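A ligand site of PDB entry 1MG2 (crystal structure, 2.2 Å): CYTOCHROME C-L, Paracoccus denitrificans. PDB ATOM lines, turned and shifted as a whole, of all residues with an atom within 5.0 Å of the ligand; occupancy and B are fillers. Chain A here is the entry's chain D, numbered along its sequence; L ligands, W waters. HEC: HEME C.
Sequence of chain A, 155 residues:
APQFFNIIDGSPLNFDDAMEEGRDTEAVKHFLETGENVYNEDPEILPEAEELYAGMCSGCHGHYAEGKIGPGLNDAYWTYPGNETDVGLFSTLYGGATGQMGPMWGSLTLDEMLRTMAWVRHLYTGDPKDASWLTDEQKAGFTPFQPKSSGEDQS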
ATOM      1  N   MET A  56       8.246  -0.054 -30.830  1.00  0.00           N
ATOM      2  CA  MET A  56       8.389  -0.713 -29.537  1.00  0.00           C
ATOM      3  C   MET A  56       8.896   0.167 -28.382  1.00  0.00           C
ATOM      4  O   MET A  56       8.615  -0.129 -27.227  1.00  0.00           O
ATOM      5  CB  MET A  56       9.325  -1.913 -29.689  1.00  0.00           C
ATOM      6  CG  MET A  56       8.862  -3.181 -29.018  1.00  0.00           C
ATOM      7  SD  MET A  56       7.462  -3.932 -29.847  1.00  0.00           S
ATOM      8  CE  MET A  56       6.215  -3.771 -28.556  1.00  0.00           C
ATOM      9  N   CYS A  57       9.624   1.237 -28.692  1.00  0.00           N
ATOM     10  CA  CYS A  57      10.206   2.058 -27.637  1.00  0.00           C
ATOM     11  C   CYS A  57      10.020   3.577 -27.672  1.00  0.00           C
ATOM     12  O   CYS A  57       9.928   4.210 -26.625  1.00  0.00           O
ATOM     13  CB  CYS A  57      11.706   1.782 -27.567  1.00  0.00           C
ATOM     14  SG  CYS A  57      12.220   0.121 -28.143  1.00  0.00           S
ATOM     15  N   CYS A  60       7.724   5.798 -25.202  1.00  0.00           N
ATOM     16  CA  CYS A  60       8.120   6.125 -23.844  1.00  0.00           C
ATOM     17  C   CYS A  60       9.506   6.762 -23.774  1.00  0.00           C
ATOM     18  O   CYS A  60       9.690   7.774 -23.084  1.00  0.00           O
ATOM     19  CB  CYS A  60       8.073   4.876 -22.962  1.00  0.00           C
ATOM     20  SG  CYS A  60       6.407   4.168 -22.691  1.00  0.00           S
ATOM     21  N   HIS A  61      10.478   6.180 -24.467  1.00  0.00           N
ATOM     22  CA  HIS A  61      11.854   6.682 -24.434  1.00  0.00           C
ATOM     23  C   HIS A  61      12.233   7.845 -25.352  1.00  0.00           C
ATOM     24  O   HIS A  61      13.332   8.396 -25.232  1.00  0.00           O
ATOM     25  CB  HIS A  61      12.818   5.516 -24.628  1.00  0.00           C
ATOM     26  CG  HIS A  61      12.890   4.608 -23.444  1.00  0.00           C
ATOM     27  ND1 HIS A  61      13.429   5.045 -22.263  1.00  0.00           N
ATOM     28  CD2 HIS A  61      12.372   3.369 -23.533  1.00  0.00           C
ATOM     29  CE1 HIS A  61      13.237   3.929 -21.468  1.00  0.00           C
ATOM     30  NE2 HIS A  61      12.585   2.896 -22.236  1.00  0.00           N
ATOM     31  N   GLY A  70       9.479   8.293 -20.494  1.00  0.00           N
ATOM     32  CA  GLY A  70      10.401   7.382 -19.850  1.00  0.00           C
ATOM     33  C   GLY A  70      11.770   8.016 -19.864  1.00  0.00           C
ATOM     34  O   GLY A  70      11.940   9.092 -20.447  1.00  0.00           O
ATOM     35  N   PRO A  71      12.773   7.376 -19.256  1.00  0.00           N
ATOM     36  CA  PRO A  71      14.146   7.908 -19.203  1.00  0.00           C
ATOM     37  C   PRO A  71      14.934   7.857 -20.511  1.00  0.00           C
ATOM     38  O   PRO A  71      14.619   7.089 -21.419  1.00  0.00           O
ATOM     39  CB  PRO A  71      14.794   7.046 -18.115  1.00  0.00           C
ATOM     40  CG  PRO A  71      14.131   5.717 -18.325  1.00  0.00           C
ATOM     41  CD  PRO A  71      12.670   6.107 -18.521  1.00  0.00           C
ATOM     42  N   GLY A  72      15.968   8.683 -20.580  1.00  0.00           N
ATOM     43  CA  GLY A  72      16.819   8.709 -21.757  1.00  0.00           C
ATOM     44  C   GLY A  72      17.681   7.460 -21.817  1.00  0.00           C
ATOM     45  O   GLY A  72      17.983   6.856 -20.780  1.00  0.00           O
ATOM     46  N   LEU A  73      18.063   7.072 -23.030  1.00  0.00           N
ATOM     47  CA  LEU A  73      18.894   5.898 -23.262  1.00  0.00           C
ATOM     48  C   LEU A  73      20.110   6.249 -24.121  1.00  0.00           C
ATOM     49  O   LEU A  73      20.966   5.396 -24.369  1.00  0.00           O
ATOM     50  CB  LEU A  73      18.062   4.833 -24.004  1.00  0.00           C
ATOM     51  CG  LEU A  73      17.146   3.840 -23.292  1.00  0.00           C
ATOM     52  CD1 LEU A  73      16.585   4.422 -22.010  1.00  0.00           C
ATOM     53  CD2 LEU A  73      16.031   3.448 -24.249  1.00  0.00           C
ATOM     54  N   TYR A  77      25.048   7.625 -18.886  1.00  0.00           N
ATOM     55  CA  TYR A  77      24.419   7.319 -17.615  1.00  0.00           C
ATOM     56  C   TYR A  77      23.359   6.231 -17.757  1.00  0.00           C
ATOM     57  O   TYR A  77      22.546   6.258 -18.671  1.00  0.00           O
ATOM     58  CB  TYR A  77      23.744   8.549 -17.015  1.00  0.00           C
ATOM     59  CG  TYR A  77      22.861   8.185 -15.857  1.00  0.00           C
ATOM     60  CD1 TYR A  77      23.411   7.752 -14.644  1.00  0.00           C
ATOM     61  CD2 TYR A  77      21.483   8.144 -15.998  1.00  0.00           C
ATOM     62  CE1 TYR A  77      22.599   7.285 -13.610  1.00  0.00           C
ATOM     63  CE2 TYR A  77      20.659   7.683 -14.964  1.00  0.00           C
ATOM     64  CZ  TYR A  77      21.227   7.260 -13.781  1.00  0.00           C
ATOM     65  OH  TYR A  77      20.415   6.773 -12.771  1.00  0.00           O
ATOM     66  N   TRP A  78      23.390   5.283 -16.825  1.00  0.00           N
ATOM     67  CA  TRP A  78      22.432   4.179 -16.789  1.00  0.00           C
ATOM     68  C   TRP A  78      22.018   3.945 -15.347  1.00  0.00           C
ATOM     69  O   TRP A  78      22.854   3.788 -14.468  1.00  0.00           O
ATOM     70  CB  TRP A  78      23.047   2.894 -17.332  1.00  0.00           C
ATOM     71  CG  TRP A  78      23.537   2.978 -18.743  1.00  0.00           C
ATOM     72  CD1 TRP A  78      24.828   3.225 -19.147  1.00  0.00           C
ATOM     73  CD2 TRP A  78      22.764   2.809 -19.933  1.00  0.00           C
ATOM     74  NE1 TRP A  78      24.883   3.215 -20.523  1.00  0.00           N
ATOM     75  CE2 TRP A  78      23.631   2.966 -21.027  1.00  0.00           C
ATOM     76  CE3 TRP A  78      21.403   2.553 -20.180  1.00  0.00           C
ATOM     77  CZ2 TRP A  78      23.197   2.865 -22.357  1.00  0.00           C
ATOM     78  CZ3 TRP A  78      20.971   2.456 -21.500  1.00  0.00           C
ATOM     79  CH2 TRP A  78      21.870   2.614 -22.568  1.00  0.00           C
ATOM     80  N   THR A  79      20.708   3.936 -15.102  1.00  0.00           N
ATOM     81  CA  THR A  79      20.205   3.693 -13.761  1.00  0.00           C
ATOM     82  C   THR A  79      20.746   2.320 -13.336  1.00  0.00           C
ATOM     83  O   THR A  79      21.121   2.097 -12.183  1.00  0.00           O
ATOM     84  CB  THR A  79      18.667   3.707 -13.761  1.00  0.00           C
ATOM     85  OG1 THR A  79      18.207   5.032 -14.069  1.00  0.00           O
ATOM     86  CG2 THR A  79      18.125   3.295 -12.415  1.00  0.00           C
ATOM     87  N   TYR A  80      20.789   1.402 -14.301  1.00  0.00           N
ATOM     88  CA  TYR A  80      21.300   0.055 -14.060  1.00  0.00           C
ATOM     89  C   TYR A  80      22.632   0.015 -14.799  1.00  0.00           C
ATOM     90  O   TYR A  80      22.701  -0.317 -15.987  1.00  0.00           O
ATOM     91  CB  TYR A  80      20.327  -0.985 -14.608  1.00  0.00           C
ATOM     92  CG  TYR A  80      18.972  -0.907 -13.926  1.00  0.00           C
ATOM     93  CD1 TYR A  80      18.804  -1.375 -12.626  1.00  0.00           C
ATOM     94  CD2 TYR A  80      17.898  -0.273 -14.551  1.00  0.00           C
ATOM     95  CE1 TYR A  80      17.606  -1.214 -11.956  1.00  0.00           C
ATOM     96  CE2 TYR A  80      16.687  -0.106 -13.881  1.00  0.00           C
ATOM     97  CZ  TYR A  80      16.550  -0.574 -12.587  1.00  0.00           C
ATOM     98  OH  TYR A  80      15.368  -0.373 -11.927  1.00  0.00           O
ATOM     99  N   ASN A  83      24.047  -1.805 -17.992  1.00  0.00           N
ATOM    100  CA  ASN A  83      23.578  -1.529 -19.329  1.00  0.00           C
ATOM    101  C   ASN A  83      24.598  -0.872 -20.243  1.00  0.00           C
ATOM    102  O   ASN A  83      24.299  -0.536 -21.383  1.00  0.00           O
ATOM    103  CB  ASN A  83      22.285  -0.714 -19.280  1.00  0.00           C
ATOM    104  CG  ASN A  83      21.109  -1.537 -18.784  1.00  0.00           C
ATOM    105  OD1 ASN A  83      21.051  -2.736 -19.024  1.00  0.00           O
ATOM    106  ND2 ASN A  83      20.159  -0.883 -18.117  1.00  0.00           N
ATOM    107  N   LEU A  89      22.352  -4.873 -21.118  1.00  0.00           N
ATOM    108  CA  LEU A  89      21.238  -4.277 -21.862  1.00  0.00           C
ATOM    109  C   LEU A  89      20.220  -5.372 -22.210  1.00  0.00           C
ATOM    110  O   LEU A  89      19.011  -5.211 -22.016  1.00  0.00           O
ATOM    111  CB  LEU A  89      21.760  -3.634 -23.154  1.00  0.00           C
ATOM    112  CG  LEU A  89      21.057  -2.361 -23.636  1.00  0.00           C
ATOM    113  CD1 LEU A  89      21.379  -2.127 -25.117  1.00  0.00           C
ATOM    114  CD2 LEU A  89      19.556  -2.500 -23.430  1.00  0.00           C
ATOM    115  N   THR A  92      18.270  -6.597 -19.369  1.00  0.00           N
ATOM    116  CA  THR A  92      17.235  -5.622 -18.997  1.00  0.00           C
ATOM    117  C   THR A  92      15.955  -5.860 -19.790  1.00  0.00           C
ATOM    118  O   THR A  92      14.867  -5.912 -19.213  1.00  0.00           O
ATOM    119  CB  THR A  92      17.703  -4.182 -19.256  1.00  0.00           C
ATOM    120  OG1 THR A  92      18.774  -3.861 -18.370  1.00  0.00           O
ATOM    121  CG2 THR A  92      16.556  -3.219 -19.024  1.00  0.00           C
ATOM    122  N   LEU A  93      16.082  -6.011 -21.105  1.00  0.00           N
ATOM    123  CA  LEU A  93      14.921  -6.237 -21.961  1.00  0.00           C
ATOM    124  C   LEU A  93      14.245  -7.571 -21.676  1.00  0.00           C
ATOM    125  O   LEU A  93      13.037  -7.631 -21.417  1.00  0.00           O
ATOM    126  CB  LEU A  93      15.307  -6.181 -23.440  1.00  0.00           C
ATOM    127  CG  LEU A  93      16.059  -4.939 -23.921  1.00  0.00           C
ATOM    128  CD1 LEU A  93      16.130  -4.943 -25.435  1.00  0.00           C
ATOM    129  CD2 LEU A  93      15.345  -3.707 -23.425  1.00  0.00           C
ATOM    130  N   ALA A  97      12.722  -4.398 -16.053  1.00  0.00           N
ATOM    131  CA  ALA A  97      13.189  -3.541 -14.970  1.00  0.00           C
ATOM    132  C   ALA A  97      12.028  -3.425 -13.987  1.00  0.00           C
ATOM    133  O   ALA A  97      11.484  -4.441 -13.548  1.00  0.00           O
ATOM    134  CB  ALA A  97      13.559  -2.184 -15.496  1.00  0.00           C
ATOM    135  N   THR A  98      11.631  -2.201 -13.649  1.00  0.00           N
ATOM    136  CA  THR A  98      10.515  -1.995 -12.736  1.00  0.00           C
ATOM    137  C   THR A  98       9.434  -1.152 -13.420  1.00  0.00           C
ATOM    138  O   THR A  98       9.658  -0.587 -14.497  1.00  0.00           O
ATOM    139  CB  THR A  98      10.945  -1.287 -11.434  1.00  0.00           C
ATOM    140  OG1 THR A  98      11.119   0.108 -11.683  1.00  0.00           O
ATOM    141  CG2 THR A  98      12.257  -1.860 -10.928  1.00  0.00           C
ATOM    142  N   GLN A 100       6.530   0.117 -15.671  1.00  0.00           N
ATOM    143  CA  GLN A 100       6.121  -0.258 -17.016  1.00  0.00           C
ATOM    144  C   GLN A 100       7.199  -0.893 -17.872  1.00  0.00           C
ATOM    145  O   GLN A 100       6.930  -1.344 -18.998  1.00  0.00           O
ATOM    146  CB  GLN A 100       5.533   0.948 -17.746  1.00  0.00           C
ATOM    147  CG  GLN A 100       4.109   1.251 -17.319  1.00  0.00           C
ATOM    148  CD  GLN A 100       3.452   2.272 -18.209  1.00  0.00           C
ATOM    149  OE1 GLN A 100       3.593   3.488 -18.004  1.00  0.00           O
ATOM    150  NE2 GLN A 100       2.730   1.797 -19.215  1.00  0.00           N
ATOM    151  N   MET A 101       8.435  -0.946 -17.373  1.00  0.00           N
ATOM    152  CA  MET A 101       9.517  -1.556 -18.130  1.00  0.00           C
ATOM    153  C   MET A 101       9.671  -2.993 -17.658  1.00  0.00           C
ATOM    154  O   MET A 101      10.599  -3.316 -16.912  1.00  0.00           O
ATOM    155  CB  MET A 101      10.823  -0.799 -17.909  1.00  0.00           C
ATOM    156  CG  MET A 101      11.952  -1.255 -18.822  1.00  0.00           C
ATOM    157  SD  MET A 101      11.641  -0.975 -20.592  1.00  0.00           S
ATOM    158  CE  MET A 101      12.540  -2.330 -21.290  1.00  0.00           C
ATOM    159  N   MET A 104      10.321  -8.655 -21.748  1.00  0.00           N
ATOM    160  CA  MET A 104       9.887  -8.662 -23.142  1.00  0.00           C
ATOM    161  C   MET A 104      10.103 -10.004 -23.827  1.00  0.00           C
ATOM    162  O   MET A 104      10.009 -10.099 -25.046  1.00  0.00           O
ATOM    163  CB  MET A 104      10.626  -7.595 -23.931  1.00  0.00           C
ATOM    164  CG  MET A 104      10.832  -6.305 -23.182  1.00  0.00           C
ATOM    165  SD  MET A 104      11.018  -4.921 -24.296  1.00  0.00           S
ATOM    166  CE  MET A 104       9.769  -3.804 -23.624  1.00  0.00           C
ATOM    167  N   LEU A 108       9.237  -9.992 -27.885  1.00  0.00           N
ATOM    168  CA  LEU A 108      10.355  -9.973 -28.821  1.00  0.00           C
ATOM    169  C   LEU A 108      11.172 -11.258 -28.823  1.00  0.00           C
ATOM    170  O   LEU A 108      11.364 -11.888 -27.775  1.00  0.00           O
ATOM    171  CB  LEU A 108      11.272  -8.786 -28.507  1.00  0.00           C
ATOM    172  CG  LEU A 108      10.708  -7.367 -28.636  1.00  0.00           C
ATOM    173  CD1 LEU A 108      11.724  -6.373 -28.110  1.00  0.00           C
ATOM    174  CD2 LEU A 108      10.361  -7.088 -30.097  1.00  0.00           C
ATOM    175  N   THR A 116      17.069  -4.440 -31.998  1.00  0.00           N
ATOM    176  CA  THR A 116      16.577  -3.248 -31.327  1.00  0.00           C
ATOM    177  C   THR A 116      17.709  -2.610 -30.518  1.00  0.00           C
ATOM    178  O   THR A 116      17.904  -1.390 -30.569  1.00  0.00           O
ATOM    179  CB  THR A 116      15.413  -3.587 -30.372  1.00  0.00           C
ATOM    180  OG1 THR A 116      14.438  -4.366 -31.070  1.00  0.00           O
ATOM    181  CG2 THR A 116      14.741  -2.310 -29.871  1.00  0.00           C
ATOM    182  N   VAL A 120      19.652   1.298 -30.311  1.00  0.00           N
ATOM    183  CA  VAL A 120      19.812   2.076 -29.100  1.00  0.00           C
ATOM    184  C   VAL A 120      21.253   2.529 -28.935  1.00  0.00           C
ATOM    185  O   VAL A 120      21.521   3.656 -28.525  1.00  0.00           O
ATOM    186  CB  VAL A 120      19.376   1.272 -27.853  1.00  0.00           C
ATOM    187  CG1 VAL A 120      19.937   1.926 -26.585  1.00  0.00           C
ATOM    188  CG2 VAL A 120      17.853   1.228 -27.774  1.00  0.00           C
HETATM  189 FE   HEC L   1      12.162   1.109 -21.440  1.00  0.00          FE
HETATM  190  CHA HEC L   1      13.942   1.745 -18.639  1.00  0.00           C
HETATM  191  CHB HEC L   1      14.983  -0.130 -22.916  1.00  0.00           C
HETATM  192  CHC HEC L   1      10.400   0.422 -24.277  1.00  0.00           C
HETATM  193  CHD HEC L   1       9.389   2.466 -20.026  1.00  0.00           C
HETATM  194  NA  HEC L   1      14.101   0.850 -20.872  1.00  0.00           N
HETATM  195  C1A HEC L   1      14.634   1.177 -19.664  1.00  0.00           C
HETATM  196  C2A HEC L   1      16.052   0.831 -19.646  1.00  0.00           C
HETATM  197  C3A HEC L   1      16.341   0.308 -20.847  1.00  0.00           C
HETATM  198  C4A HEC L   1      15.120   0.311 -21.638  1.00  0.00           C
HETATM  199  CMA HEC L   1      17.702  -0.203 -21.346  1.00  0.00           C
HETATM  200  CAA HEC L   1      16.997   1.065 -18.442  1.00  0.00           C
HETATM  201  CBA HEC L   1      17.940   2.267 -18.674  1.00  0.00           C
HETATM  202  CGA HEC L   1      18.854   2.610 -17.512  1.00  0.00           C
HETATM  203  O1A HEC L   1      19.624   1.667 -17.113  1.00  0.00           O
HETATM  204  O2A HEC L   1      18.822   3.751 -17.050  1.00  0.00           O
HETATM  205  NB  HEC L   1      12.587   0.312 -23.234  1.00  0.00           N
HETATM  206  C1B HEC L   1      13.834  -0.142 -23.648  1.00  0.00           C
HETATM  207  C2B HEC L   1      13.760  -0.651 -25.007  1.00  0.00           C
HETATM  208  C3B HEC L   1      12.460  -0.517 -25.386  1.00  0.00           C
HETATM  209  C4B HEC L   1      11.740   0.095 -24.298  1.00  0.00           C
HETATM  210  CMB HEC L   1      14.930  -1.234 -25.805  1.00  0.00           C
HETATM  211  CAB HEC L   1      11.804  -0.900 -26.713  1.00  0.00           C
HETATM  212  CBB HEC L   1      11.774  -2.418 -26.971  1.00  0.00           C
HETATM  213  NC  HEC L   1      10.274   1.380 -22.012  1.00  0.00           N
HETATM  214  C1C HEC L   1       9.733   1.033 -23.233  1.00  0.00           C
HETATM  215  C2C HEC L   1       8.327   1.427 -23.296  1.00  0.00           C
HETATM  216  C3C HEC L   1       8.040   2.010 -22.123  1.00  0.00           C
HETATM  217  C4C HEC L   1       9.242   1.981 -21.316  1.00  0.00           C
HETATM  218  CMC HEC L   1       7.405   1.194 -24.528  1.00  0.00           C
HETATM  219  CAC HEC L   1       6.725   2.652 -21.680  1.00  0.00           C
HETATM  220  CBC HEC L   1       5.524   1.700 -21.511  1.00  0.00           C
HETATM  221  ND  HEC L   1      11.747   1.929 -19.692  1.00  0.00           N
HETATM  222  C1D HEC L   1      10.523   2.439 -19.252  1.00  0.00           C
HETATM  223  C2D HEC L   1      10.651   2.931 -17.884  1.00  0.00           C
HETATM  224  C3D HEC L   1      11.940   2.712 -17.499  1.00  0.00           C
HETATM  225  C4D HEC L   1      12.613   2.100 -18.622  1.00  0.00           C
HETATM  226  CMD HEC L   1       9.519   3.567 -17.051  1.00  0.00           C
HETATM  227  CAD HEC L   1      12.587   3.018 -16.147  1.00  0.00           C
HETATM  228  CBD HEC L   1      12.676   1.619 -15.412  1.00  0.00           C
HETATM  229  CGD HEC L   1      13.314   1.586 -14.050  1.00  0.00           C
HETATM  230  O1D HEC L   1      13.070   0.625 -13.304  1.00  0.00           O
HETATM  231  O2D HEC L   1      14.077   2.528 -13.785  1.00  0.00           O
HETATM  232  O   HOH W   1       6.736   2.823 -15.069  1.00  0.00           O
HETATM  233  O   HOH W   2      13.269   3.482 -10.542  1.00  0.00           O
HETATM  234  O   HOH W   3      15.320   5.144 -14.778  1.00  0.00           O
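O of Cys 60 sits at hydrogen-bond distance from N of Gly 70 (2.6 Å).
The backbone carbonyl oxygen (O) of Pro 71 is in hydrogen-bond range of a ring nitrogen (ND1) of His 61 (2.5 Å).
OG1 of Thr 79 is in hydrogen-bond range of OH of Tyr 77, 3.1 Å away.
The side-chain amide nitrogen (ND2) of Asn 83 lies close to the backbone carbonyl oxygen (O) of Tyr 80, 3.4 Å away.
N of Leu 89 lies close to OD1 of Asn 83 (3.3 Å).
OD1 of Asn 83 sits at hydrogen-bond distance from OG1 of Thr 92 (2.6 Å).
The backbone carbonyl oxygen of Leu 93 sits at hydrogen-bond distance from the backbone NH of Met 104, at 2.9 Å.
A carbon (CAB) of the ligand is covalently linked to the side-chain sulfur (SG) of Cys 57 (1.8 Å).
The side-chain sulfur of Cys 60 is covalently linked to a carbon (CAC) of the ligand.
A ring nitrogen (NE2) of His 61 binds an iron atom (FE) of the ligand, 2.0 Å away.
SD of Met 101 is bound to FE of the ligand.
An oxygen (O1D) of the ligand sits close to the backbone NH of Thr 98, 3.2 Å away.
An oxygen (O1D) of the ligand lies close to the side-chain hydroxyl (OG1) of Thr 98.
The backbone NH (N) of Thr 79 lies close to an oxygen (O2A) of the ligand.
An oxygen (O2A) of the ligand lies close to the side-chain hydroxyl (OG1) of Thr 79, 3.3 Å away.
O1A of the ligand lies close to ND2 of Asn 83 (2.8 Å).
N of Tyr 80 lies close to O1A of the ligand (3.1 Å).
OH of Tyr 80 sits close to O1D of the ligand (2.9 Å).
O of Met 56 touches CMC of the ligand, 3.2 Å away.
Pro 71 touches the ligand (CD to C3D, 3.6 Å).
Leu 73 touches the ligand.
Trp 78 touches the ligand.
Leu 89 touches the ligand.
Thr 92 touches the ligand (CG2 to CMA, 3.98 Å).
Leu 93 touches the ligand.
Ala 97 touches the ligand.
Gln 100 touches the ligand.
Met 104 touches the ligand.
Hydrophobic or aromatic side chains within 4 Å of the ligand: Met 56, His 61, Pro 71, Leu 73, Trp 78, Tyr 80, Leu 89, Leu 93, Ala 97, Met 101 and Met 104.
18 residues have an atom within 4 Å of the ligand: Met 56, Cys 57, Cys 60, His 61, Pro 71, Leu 73, Trp 78, Thr 79, Tyr 80, Asn 83, Leu 89, Thr 92, Leu 93, Ala 97, Thr 98, Gln 100, Met 101 and Met 104.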
